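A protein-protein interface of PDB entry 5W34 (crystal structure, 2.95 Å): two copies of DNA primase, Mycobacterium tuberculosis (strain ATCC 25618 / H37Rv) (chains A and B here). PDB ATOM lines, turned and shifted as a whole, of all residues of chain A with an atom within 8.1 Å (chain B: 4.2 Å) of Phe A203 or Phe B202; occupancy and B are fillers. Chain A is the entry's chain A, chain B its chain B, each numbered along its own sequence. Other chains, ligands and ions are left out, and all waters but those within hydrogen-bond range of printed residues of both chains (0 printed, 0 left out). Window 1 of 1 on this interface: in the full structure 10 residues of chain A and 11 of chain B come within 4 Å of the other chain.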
ATOM      1  N   HIS A 155      -8.064  -9.000 -27.073  1.00  0.00           N
ATOM      2  CA  HIS A 155      -8.882  -8.572 -25.926  1.00  0.00           C
ATOM      3  C   HIS A 155      -9.910  -7.524 -26.347  1.00  0.00           C
ATOM      4  O   HIS A 155     -10.086  -6.489 -25.697  1.00  0.00           O
ATOM      5  CB  HIS A 155      -8.001  -8.074 -24.775  1.00  0.00           C
ATOM      6  CG  HIS A 155      -6.848  -8.973 -24.479  1.00  0.00           C
ATOM      7  ND1 HIS A 155      -7.005 -10.219 -23.910  1.00  0.00           N
ATOM      8  CD2 HIS A 155      -5.522  -8.822 -24.698  1.00  0.00           C
ATOM      9  CE1 HIS A 155      -5.822 -10.794 -23.786  1.00  0.00           C
ATOM     10  NE2 HIS A 155      -4.906  -9.968 -24.259  1.00  0.00           N
ATOM     11  N   LEU A 193     -18.587 -14.138 -24.986  1.00  0.00           N
ATOM     12  CA  LEU A 193     -17.534 -13.194 -25.391  1.00  0.00           C
ATOM     13  C   LEU A 193     -16.702 -12.689 -24.211  1.00  0.00           C
ATOM     14  O   LEU A 193     -15.506 -12.447 -24.355  1.00  0.00           O
ATOM     15  CB  LEU A 193     -18.133 -12.009 -26.152  1.00  0.00           C
ATOM     16  CG  LEU A 193     -18.867 -12.328 -27.457  1.00  0.00           C
ATOM     17  CD1 LEU A 193     -19.480 -11.056 -28.018  1.00  0.00           C
ATOM     18  CD2 LEU A 193     -17.955 -12.973 -28.488  1.00  0.00           C
ATOM     19  N   ARG A 194     -17.337 -12.527 -23.053  1.00  0.00           N
ATOM     20  CA  ARG A 194     -16.633 -12.190 -21.812  1.00  0.00           C
ATOM     21  C   ARG A 194     -15.627 -13.290 -21.452  1.00  0.00           C
ATOM     22  O   ARG A 194     -14.489 -12.995 -21.110  1.00  0.00           O
ATOM     23  CB  ARG A 194     -17.652 -11.979 -20.682  1.00  0.00           C
ATOM     24  CG  ARG A 194     -17.083 -11.692 -19.293  1.00  0.00           C
ATOM     25  CD  ARG A 194     -18.175 -11.715 -18.224  1.00  0.00           C
ATOM     26  NE  ARG A 194     -19.056 -12.891 -18.341  1.00  0.00           N
ATOM     27  CZ  ARG A 194     -18.908 -14.066 -17.717  1.00  0.00           C
ATOM     28  NH1 ARG A 194     -17.910 -14.293 -16.866  1.00  0.00           N
ATOM     29  NH2 ARG A 194     -19.791 -15.035 -17.944  1.00  0.00           N
ATOM     30  N   ARG A 195     -16.061 -14.548 -21.547  1.00  0.00           N
ATOM     31  CA  ARG A 195     -15.203 -15.721 -21.286  1.00  0.00           C
ATOM     32  C   ARG A 195     -13.942 -15.772 -22.145  1.00  0.00           C
ATOM     33  O   ARG A 195     -12.838 -15.896 -21.615  1.00  0.00           O
ATOM     34  CB  ARG A 195     -15.991 -17.033 -21.453  1.00  0.00           C
ATOM     35  CG  ARG A 195     -16.385 -17.683 -20.136  1.00  0.00           C
ATOM     36  CD  ARG A 195     -15.294 -18.605 -19.585  1.00  0.00           C
ATOM     37  NE  ARG A 195     -14.915 -18.283 -18.208  1.00  0.00           N
ATOM     38  CZ  ARG A 195     -15.714 -18.375 -17.140  1.00  0.00           C
ATOM     39  NH1 ARG A 195     -15.238 -18.051 -15.938  1.00  0.00           N
ATOM     40  NH2 ARG A 195     -16.983 -18.774 -17.254  1.00  0.00           N
ATOM     41  N   MET A 197     -12.276 -13.488 -23.695  1.00  0.00           N
ATOM     42  CA  MET A 197     -11.319 -12.409 -23.415  1.00  0.00           C
ATOM     43  C   MET A 197     -10.614 -12.488 -22.055  1.00  0.00           C
ATOM     44  O   MET A 197      -9.671 -11.731 -21.806  1.00  0.00           O
ATOM     45  CB  MET A 197     -12.013 -11.056 -23.574  1.00  0.00           C
ATOM     46  CG  MET A 197     -12.494 -10.825 -24.998  1.00  0.00           C
ATOM     47  SD  MET A 197     -13.166  -9.187 -25.289  1.00  0.00           S
ATOM     48  CE  MET A 197     -14.841  -9.350 -24.679  1.00  0.00           C
ATOM     49  N   MET A 198     -11.056 -13.395 -21.186  1.00  0.00           N
ATOM     50  CA  MET A 198     -10.411 -13.609 -19.886  1.00  0.00           C
ATOM     51  C   MET A 198      -9.079 -14.345 -20.001  1.00  0.00           C
ATOM     52  O   MET A 198      -8.076 -13.914 -19.426  1.00  0.00           O
ATOM     53  CB  MET A 198     -11.324 -14.411 -18.955  1.00  0.00           C
ATOM     54  CG  MET A 198     -12.674 -13.769 -18.695  1.00  0.00           C
ATOM     55  SD  MET A 198     -13.000 -13.575 -16.940  1.00  0.00           S
ATOM     56  CE  MET A 198     -14.739 -13.961 -16.900  1.00  0.00           C
ATOM     57  N   ASP A 199      -9.081 -15.442 -20.757  1.00  0.00           N
ATOM     58  CA  ASP A 199      -7.988 -16.423 -20.728  1.00  0.00           C
ATOM     59  C   ASP A 199      -6.729 -15.904 -21.420  1.00  0.00           C
ATOM     60  O   ASP A 199      -5.716 -15.640 -20.767  1.00  0.00           O
ATOM     61  CB  ASP A 199      -8.433 -17.744 -21.373  1.00  0.00           C
ATOM     62  CG  ASP A 199      -9.744 -18.271 -20.797  1.00  0.00           C
ATOM     63  OD1 ASP A 199      -9.986 -18.092 -19.583  1.00  0.00           O
ATOM     64  OD2 ASP A 199     -10.536 -18.861 -21.563  1.00  0.00           O
ATOM     65  N   PHE A 202      -5.024 -13.124 -18.517  1.00  0.00           N
ATOM     66  CA  PHE A 202      -4.683 -11.846 -19.158  1.00  0.00           C
ATOM     67  C   PHE A 202      -5.633 -10.706 -18.722  1.00  0.00           C
ATOM     68  O   PHE A 202      -5.311  -9.528 -18.912  1.00  0.00           O
ATOM     69  CB  PHE A 202      -4.654 -12.007 -20.690  1.00  0.00           C
ATOM     70  CG  PHE A 202      -3.364 -11.546 -21.338  1.00  0.00           C
ATOM     71  CD1 PHE A 202      -2.323 -12.447 -21.571  1.00  0.00           C
ATOM     72  CD2 PHE A 202      -3.192 -10.218 -21.724  1.00  0.00           C
ATOM     73  CE1 PHE A 202      -1.138 -12.029 -22.170  1.00  0.00           C
ATOM     74  CE2 PHE A 202      -2.012  -9.797 -22.330  1.00  0.00           C
ATOM     75  CZ  PHE A 202      -0.983 -10.702 -22.551  1.00  0.00           C
ATOM     76  N   PHE A 203      -6.800 -11.069 -18.173  1.00  0.00           N
ATOM     77  CA  PHE A 203      -7.620 -10.216 -17.272  1.00  0.00           C
ATOM     78  C   PHE A 203      -8.639  -9.258 -17.923  1.00  0.00           C
ATOM     79  O   PHE A 203      -9.847  -9.472 -17.790  1.00  0.00           O
ATOM     80  CB  PHE A 203      -6.746  -9.471 -16.239  1.00  0.00           C
ATOM     81  CG  PHE A 203      -5.756 -10.362 -15.525  1.00  0.00           C
ATOM     82  CD1 PHE A 203      -6.192 -11.490 -14.828  1.00  0.00           C
ATOM     83  CD2 PHE A 203      -4.387 -10.087 -15.559  1.00  0.00           C
ATOM     84  CE1 PHE A 203      -5.287 -12.322 -14.177  1.00  0.00           C
ATOM     85  CE2 PHE A 203      -3.479 -10.917 -14.910  1.00  0.00           C
ATOM     86  CZ  PHE A 203      -3.930 -12.033 -14.216  1.00  0.00           C
ATOM     87  N   ARG A 204      -8.169  -8.218 -18.611  1.00  0.00           N
ATOM     88  CA  ARG A 204      -9.059  -7.149 -19.122  1.00  0.00           C
ATOM     89  C   ARG A 204      -9.903  -7.586 -20.342  1.00  0.00           C
ATOM     90  O   ARG A 204     -10.040  -8.787 -20.604  1.00  0.00           O
ATOM     91  CB  ARG A 204      -8.234  -5.880 -19.421  1.00  0.00           C
ATOM     92  CG  ARG A 204      -7.365  -5.925 -20.675  1.00  0.00           C
ATOM     93  CD  ARG A 204      -6.743  -4.570 -20.964  1.00  0.00           C
ATOM     94  NE  ARG A 204      -6.029  -4.544 -22.245  1.00  0.00           N
ATOM     95  CZ  ARG A 204      -6.590  -4.401 -23.452  1.00  0.00           C
ATOM     96  NH1 ARG A 204      -5.813  -4.391 -24.535  1.00  0.00           N
ATOM     97  NH2 ARG A 204      -7.910  -4.272 -23.605  1.00  0.00           N
ATOM     98  N   GLY A 205     -10.480  -6.619 -21.064  1.00  0.00           N
ATOM     99  CA  GLY A 205     -11.145  -6.885 -22.345  1.00  0.00           C
ATOM    100  C   GLY A 205     -12.196  -5.850 -22.697  1.00  0.00           C
ATOM    101  O   GLY A 205     -13.129  -5.646 -21.927  1.00  0.00           O
ATOM    102  N   GLU A 206     -12.043  -5.198 -23.854  1.00  0.00           N
ATOM    103  CA  GLU A 206     -13.051  -4.258 -24.378  1.00  0.00           C
ATOM    104  C   GLU A 206     -14.209  -5.001 -25.034  1.00  0.00           C
ATOM    105  O   GLU A 206     -14.120  -6.200 -25.279  1.00  0.00           O
ATOM    106  CB  GLU A 206     -12.435  -3.312 -25.410  1.00  0.00           C
ATOM    107  CG  GLU A 206     -11.413  -2.337 -24.846  1.00  0.00           C
ATOM    108  CD  GLU A 206     -11.000  -1.266 -25.844  1.00  0.00           C
ATOM    109  OE1 GLU A 206      -9.922  -0.661 -25.649  1.00  0.00           O
ATOM    110  OE2 GLU A 206     -11.745  -1.017 -26.822  1.00  0.00           O
ATOM    111  N   LYS A 230     -21.354  -4.578 -14.556  1.00  0.00           N
ATOM    112  CA  LYS A 230     -19.989  -4.049 -14.397  1.00  0.00           C
ATOM    113  C   LYS A 230     -19.097  -4.257 -15.637  1.00  0.00           C
ATOM    114  O   LYS A 230     -17.950  -3.805 -15.654  1.00  0.00           O
ATOM    115  CB  LYS A 230     -19.339  -4.591 -13.103  1.00  0.00           C
ATOM    116  CG  LYS A 230     -19.511  -3.666 -11.892  1.00  0.00           C
ATOM    117  CD  LYS A 230     -20.217  -4.328 -10.716  1.00  0.00           C
ATOM    118  CE  LYS A 230     -20.350  -3.364  -9.544  1.00  0.00           C
ATOM    119  NZ  LYS A 230     -21.325  -3.852  -8.530  1.00  0.00           N
ATOM    120  N   LEU A 231     -19.626  -4.920 -16.669  1.00  0.00           N
ATOM    121  CA  LEU A 231     -19.035  -4.869 -18.017  1.00  0.00           C
ATOM    122  C   LEU A 231     -19.330  -3.552 -18.759  1.00  0.00           C
ATOM    123  O   LEU A 231     -18.705  -3.279 -19.788  1.00  0.00           O
ATOM    124  CB  LEU A 231     -19.475  -6.069 -18.881  1.00  0.00           C
ATOM    125  CG  LEU A 231     -18.487  -7.240 -18.940  1.00  0.00           C
ATOM    126  CD1 LEU A 231     -18.449  -7.977 -17.610  1.00  0.00           C
ATOM    127  CD2 LEU A 231     -18.827  -8.190 -20.081  1.00  0.00           C
ATOM    128  N   ALA A 232     -20.269  -2.746 -18.249  1.00  0.00           N
ATOM    129  CA  ALA A 232     -20.559  -1.412 -18.812  1.00  0.00           C
ATOM    130  C   ALA A 232     -19.391  -0.415 -18.708  1.00  0.00           C
ATOM    131  O   ALA A 232     -19.368   0.579 -19.437  1.00  0.00           O
ATOM    132  CB  ALA A 232     -21.813  -0.823 -18.177  1.00  0.00           C
ATOM    133  N   GLN A 234     -16.330  -1.546 -19.450  1.00  0.00           N
ATOM    134  CA  GLN A 234     -15.606  -2.027 -20.639  1.00  0.00           C
ATOM    135  C   GLN A 234     -16.439  -2.077 -21.940  1.00  0.00           C
ATOM    136  O   GLN A 234     -15.926  -2.500 -22.979  1.00  0.00           O
ATOM    137  CB  GLN A 234     -15.004  -3.415 -20.359  1.00  0.00           C
ATOM    138  CG  GLN A 234     -13.743  -3.403 -19.500  1.00  0.00           C
ATOM    139  CD  GLN A 234     -14.024  -3.218 -18.020  1.00  0.00           C
ATOM    140  OE1 GLN A 234     -14.856  -3.920 -17.441  1.00  0.00           O
ATOM    141  NE2 GLN A 234     -13.319  -2.279 -17.396  1.00  0.00           N
ATOM    142  N   ARG B 194      -1.807  -6.455  -7.923  1.00  0.00           N
ATOM    143  CA  ARG B 194      -2.817  -6.723  -8.952  1.00  0.00           C
ATOM    144  C   ARG B 194      -4.125  -7.255  -8.358  1.00  0.00           C
ATOM    145  O   ARG B 194      -5.203  -6.846  -8.783  1.00  0.00           O
ATOM    146  CB  ARG B 194      -2.265  -7.720  -9.982  1.00  0.00           C
ATOM    147  CG  ARG B 194      -3.133  -7.909 -11.221  1.00  0.00           C
ATOM    148  CD  ARG B 194      -2.689  -9.079 -12.092  1.00  0.00           C
ATOM    149  NE  ARG B 194      -2.413 -10.305 -11.335  1.00  0.00           N
ATOM    150  CZ  ARG B 194      -3.330 -11.099 -10.773  1.00  0.00           C
ATOM    151  NH1 ARG B 194      -4.634 -10.828 -10.853  1.00  0.00           N
ATOM    152  NH2 ARG B 194      -2.936 -12.185 -10.108  1.00  0.00           N
ATOM    153  N   MET B 198      -8.206  -5.624  -8.548  1.00  0.00           N
ATOM    154  CA  MET B 198      -9.244  -6.391  -9.243  1.00  0.00           C
ATOM    155  C   MET B 198     -10.636  -6.071  -8.711  1.00  0.00           C
ATOM    156  O   MET B 198     -10.825  -5.899  -7.507  1.00  0.00           O
ATOM    157  CB  MET B 198      -9.019  -7.906  -9.127  1.00  0.00           C
ATOM    158  CG  MET B 198      -7.914  -8.464 -10.011  1.00  0.00           C
ATOM    159  SD  MET B 198      -8.169 -10.201 -10.426  1.00  0.00           S
ATOM    160  CE  MET B 198      -8.146 -10.971  -8.806  1.00  0.00           C
ATOM    161  N   ASP B 199     -11.593  -5.988  -9.631  1.00  0.00           N
ATOM    162  CA  ASP B 199     -13.009  -5.860  -9.293  1.00  0.00           C
ATOM    163  C   ASP B 199     -13.831  -6.712 -10.266  1.00  0.00           C
ATOM    164  O   ASP B 199     -13.685  -6.587 -11.485  1.00  0.00           O
ATOM    165  CB  ASP B 199     -13.459  -4.386  -9.309  1.00  0.00           C
ATOM    166  CG  ASP B 199     -13.247  -3.705 -10.660  1.00  0.00           C
ATOM    167  OD1 ASP B 199     -12.214  -3.955 -11.315  1.00  0.00           O
ATOM    168  OD2 ASP B 199     -14.121  -2.909 -11.064  1.00  0.00           O
ATOM    169  N   ASP B 200     -14.660  -7.600  -9.713  1.00  0.00           N
ATOM    170  CA  ASP B 200     -15.544  -8.478 -10.495  1.00  0.00           C
ATOM    171  C   ASP B 200     -14.771  -9.363 -11.484  1.00  0.00           C
ATOM    172  O   ASP B 200     -15.190  -9.535 -12.631  1.00  0.00           O
ATOM    173  CB  ASP B 200     -16.613  -7.651 -11.229  1.00  0.00           C
ATOM    174  CG  ASP B 200     -17.265  -6.607 -10.337  1.00  0.00           C
ATOM    175  OD1 ASP B 200     -17.908  -6.991  -9.338  1.00  0.00           O
ATOM    176  OD2 ASP B 200     -17.132  -5.402 -10.637  1.00  0.00           O
ATOM    177  N   SER B 201     -13.650  -9.921 -11.020  1.00  0.00           N
ATOM    178  CA  SER B 201     -12.744 -10.750 -11.838  1.00  0.00           C
ATOM    179  C   SER B 201     -12.116 -10.005 -13.033  1.00  0.00           C
ATOM    180  O   SER B 201     -11.836 -10.614 -14.070  1.00  0.00           O
ATOM    181  CB  SER B 201     -13.452 -12.031 -12.316  1.00  0.00           C
ATOM    182  OG  SER B 201     -14.221 -12.619 -11.280  1.00  0.00           O
ATOM    183  N   PHE B 202     -11.891  -8.698 -12.872  1.00  0.00           N
ATOM    184  CA  PHE B 202     -11.261  -7.853 -13.899  1.00  0.00           C
ATOM    185  C   PHE B 202     -10.279  -6.881 -13.257  1.00  0.00           C
ATOM    186  O   PHE B 202     -10.601  -6.262 -12.242  1.00  0.00           O
ATOM    187  CB  PHE B 202     -12.308  -7.033 -14.660  1.00  0.00           C
ATOM    188  CG  PHE B 202     -13.333  -7.863 -15.373  1.00  0.00           C
ATOM    189  CD1 PHE B 202     -12.948  -8.761 -16.363  1.00  0.00           C
ATOM    190  CD2 PHE B 202     -14.686  -7.736 -15.072  1.00  0.00           C
ATOM    191  CE1 PHE B 202     -13.889  -9.532 -17.028  1.00  0.00           C
ATOM    192  CE2 PHE B 202     -15.632  -8.503 -15.734  1.00  0.00           C
ATOM    193  CZ  PHE B 202     -15.233  -9.403 -16.713  1.00  0.00           C
ATOM    194  N   PHE B 203      -9.096  -6.742 -13.860  1.00  0.00           N
ATOM    195  CA  PHE B 203      -8.121  -5.722 -13.462  1.00  0.00           C
ATOM    196  C   PHE B 203      -8.376  -4.452 -14.273  1.00  0.00           C
ATOM    197  O   PHE B 203      -8.506  -4.513 -15.498  1.00  0.00           O
ATOM    198  CB  PHE B 203      -6.691  -6.208 -13.700  1.00  0.00           C
ATOM    199  CG  PHE B 203      -5.642  -5.195 -13.336  1.00  0.00           C
ATOM    200  CD1 PHE B 203      -5.108  -5.155 -12.051  1.00  0.00           C
ATOM    201  CD2 PHE B 203      -5.201  -4.262 -14.271  1.00  0.00           C
ATOM    202  CE1 PHE B 203      -4.139  -4.216 -11.714  1.00  0.00           C
ATOM    203  CE2 PHE B 203      -4.237  -3.319 -13.936  1.00  0.00           C
ATOM    204  CZ  PHE B 203      -3.702  -3.297 -12.657  1.00  0.00           C
ATOM    205  N   ARG B 204      -8.434  -3.311 -13.586  1.00  0.00           N
ATOM    206  CA  ARG B 204      -8.722  -2.020 -14.232  1.00  0.00           C
ATOM    207  C   ARG B 204      -7.770  -0.860 -13.913  1.00  0.00           C
ATOM    208  O   ARG B 204      -7.695   0.091 -14.693  1.00  0.00           O
ATOM    209  CB  ARG B 204     -10.162  -1.598 -13.918  1.00  0.00           C
ATOM    210  CG  ARG B 204     -10.446  -1.365 -12.440  1.00  0.00           C
ATOM    211  CD  ARG B 204     -11.865  -0.877 -12.196  1.00  0.00           C
ATOM    212  NE  ARG B 204     -12.057   0.513 -12.632  1.00  0.00           N
ATOM    213  CZ  ARG B 204     -12.882   1.404 -12.073  1.00  0.00           C
ATOM    214  NH1 ARG B 204     -13.625   1.106 -11.006  1.00  0.00           N
ATOM    215  NH2 ARG B 204     -12.952   2.633 -12.582  1.00  0.00           N
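The backbone carbonyl oxygen (O) of Met A198 sits at hydrogen-bond distance from the backbone NH (N) of Phe A203. The side-chain sulfur (SD) of Met B198 sits at hydrogen-bond distance from the guanidinium group (NH1) of Arg B194 (3.6 Å).
Among the printed residues, pairs that only touch across the chains: Lys A230 with Asp B200 (3.2 Å), Leu A231 with Phe B202 (3.4 Å), Phe A203 with Arg B194 (3.5 Å), Phe A203 with Phe B202 (3.5 Å) and Arg A194 with Phe B202 (3.9 Å).
Phe A203 touches just these residues of chain B: Arg B194 (3.5 Å) and Phe B202 (3.5 Å). Of chain A, only Arg A194, Phe A203 and Leu A231 come within 4 Å of Phe B202. Of the printed residues of chain A, Arg B194 touches Phe A203. Printed residues of chain B within 4 Å of Leu A231: Phe B202 (3.4 Å). Printed residues of chain A within 4 Å of Asp B200: Lys A230 (3.2 Å). Printed residues of chain B within 4 Å of Arg A194: Phe B202 (3.9 Å). Of the printed residues of chain B, Lys A230 touches Asp B200. His A155 touches none of the printed residues of chain B. The nearest residue of chain A that does not touch Phe B202 is Met A198 (4.1 Å).
Among the printed residues, 5 pairs touch across the chains.
Arg A194 touches Phe B202, but with the chains exchanged Phe A202 does not touch Arg B194 (7.3 Å). Phe A203 touches Arg B194, but with the chains exchanged Arg A194 does not touch Phe B203 (10.9 Å). Phe A203 touches Phe B202, but with the chains exchanged Phe A202 does not touch Phe B203 (6.3 Å). 6 positions are printed for both chains.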
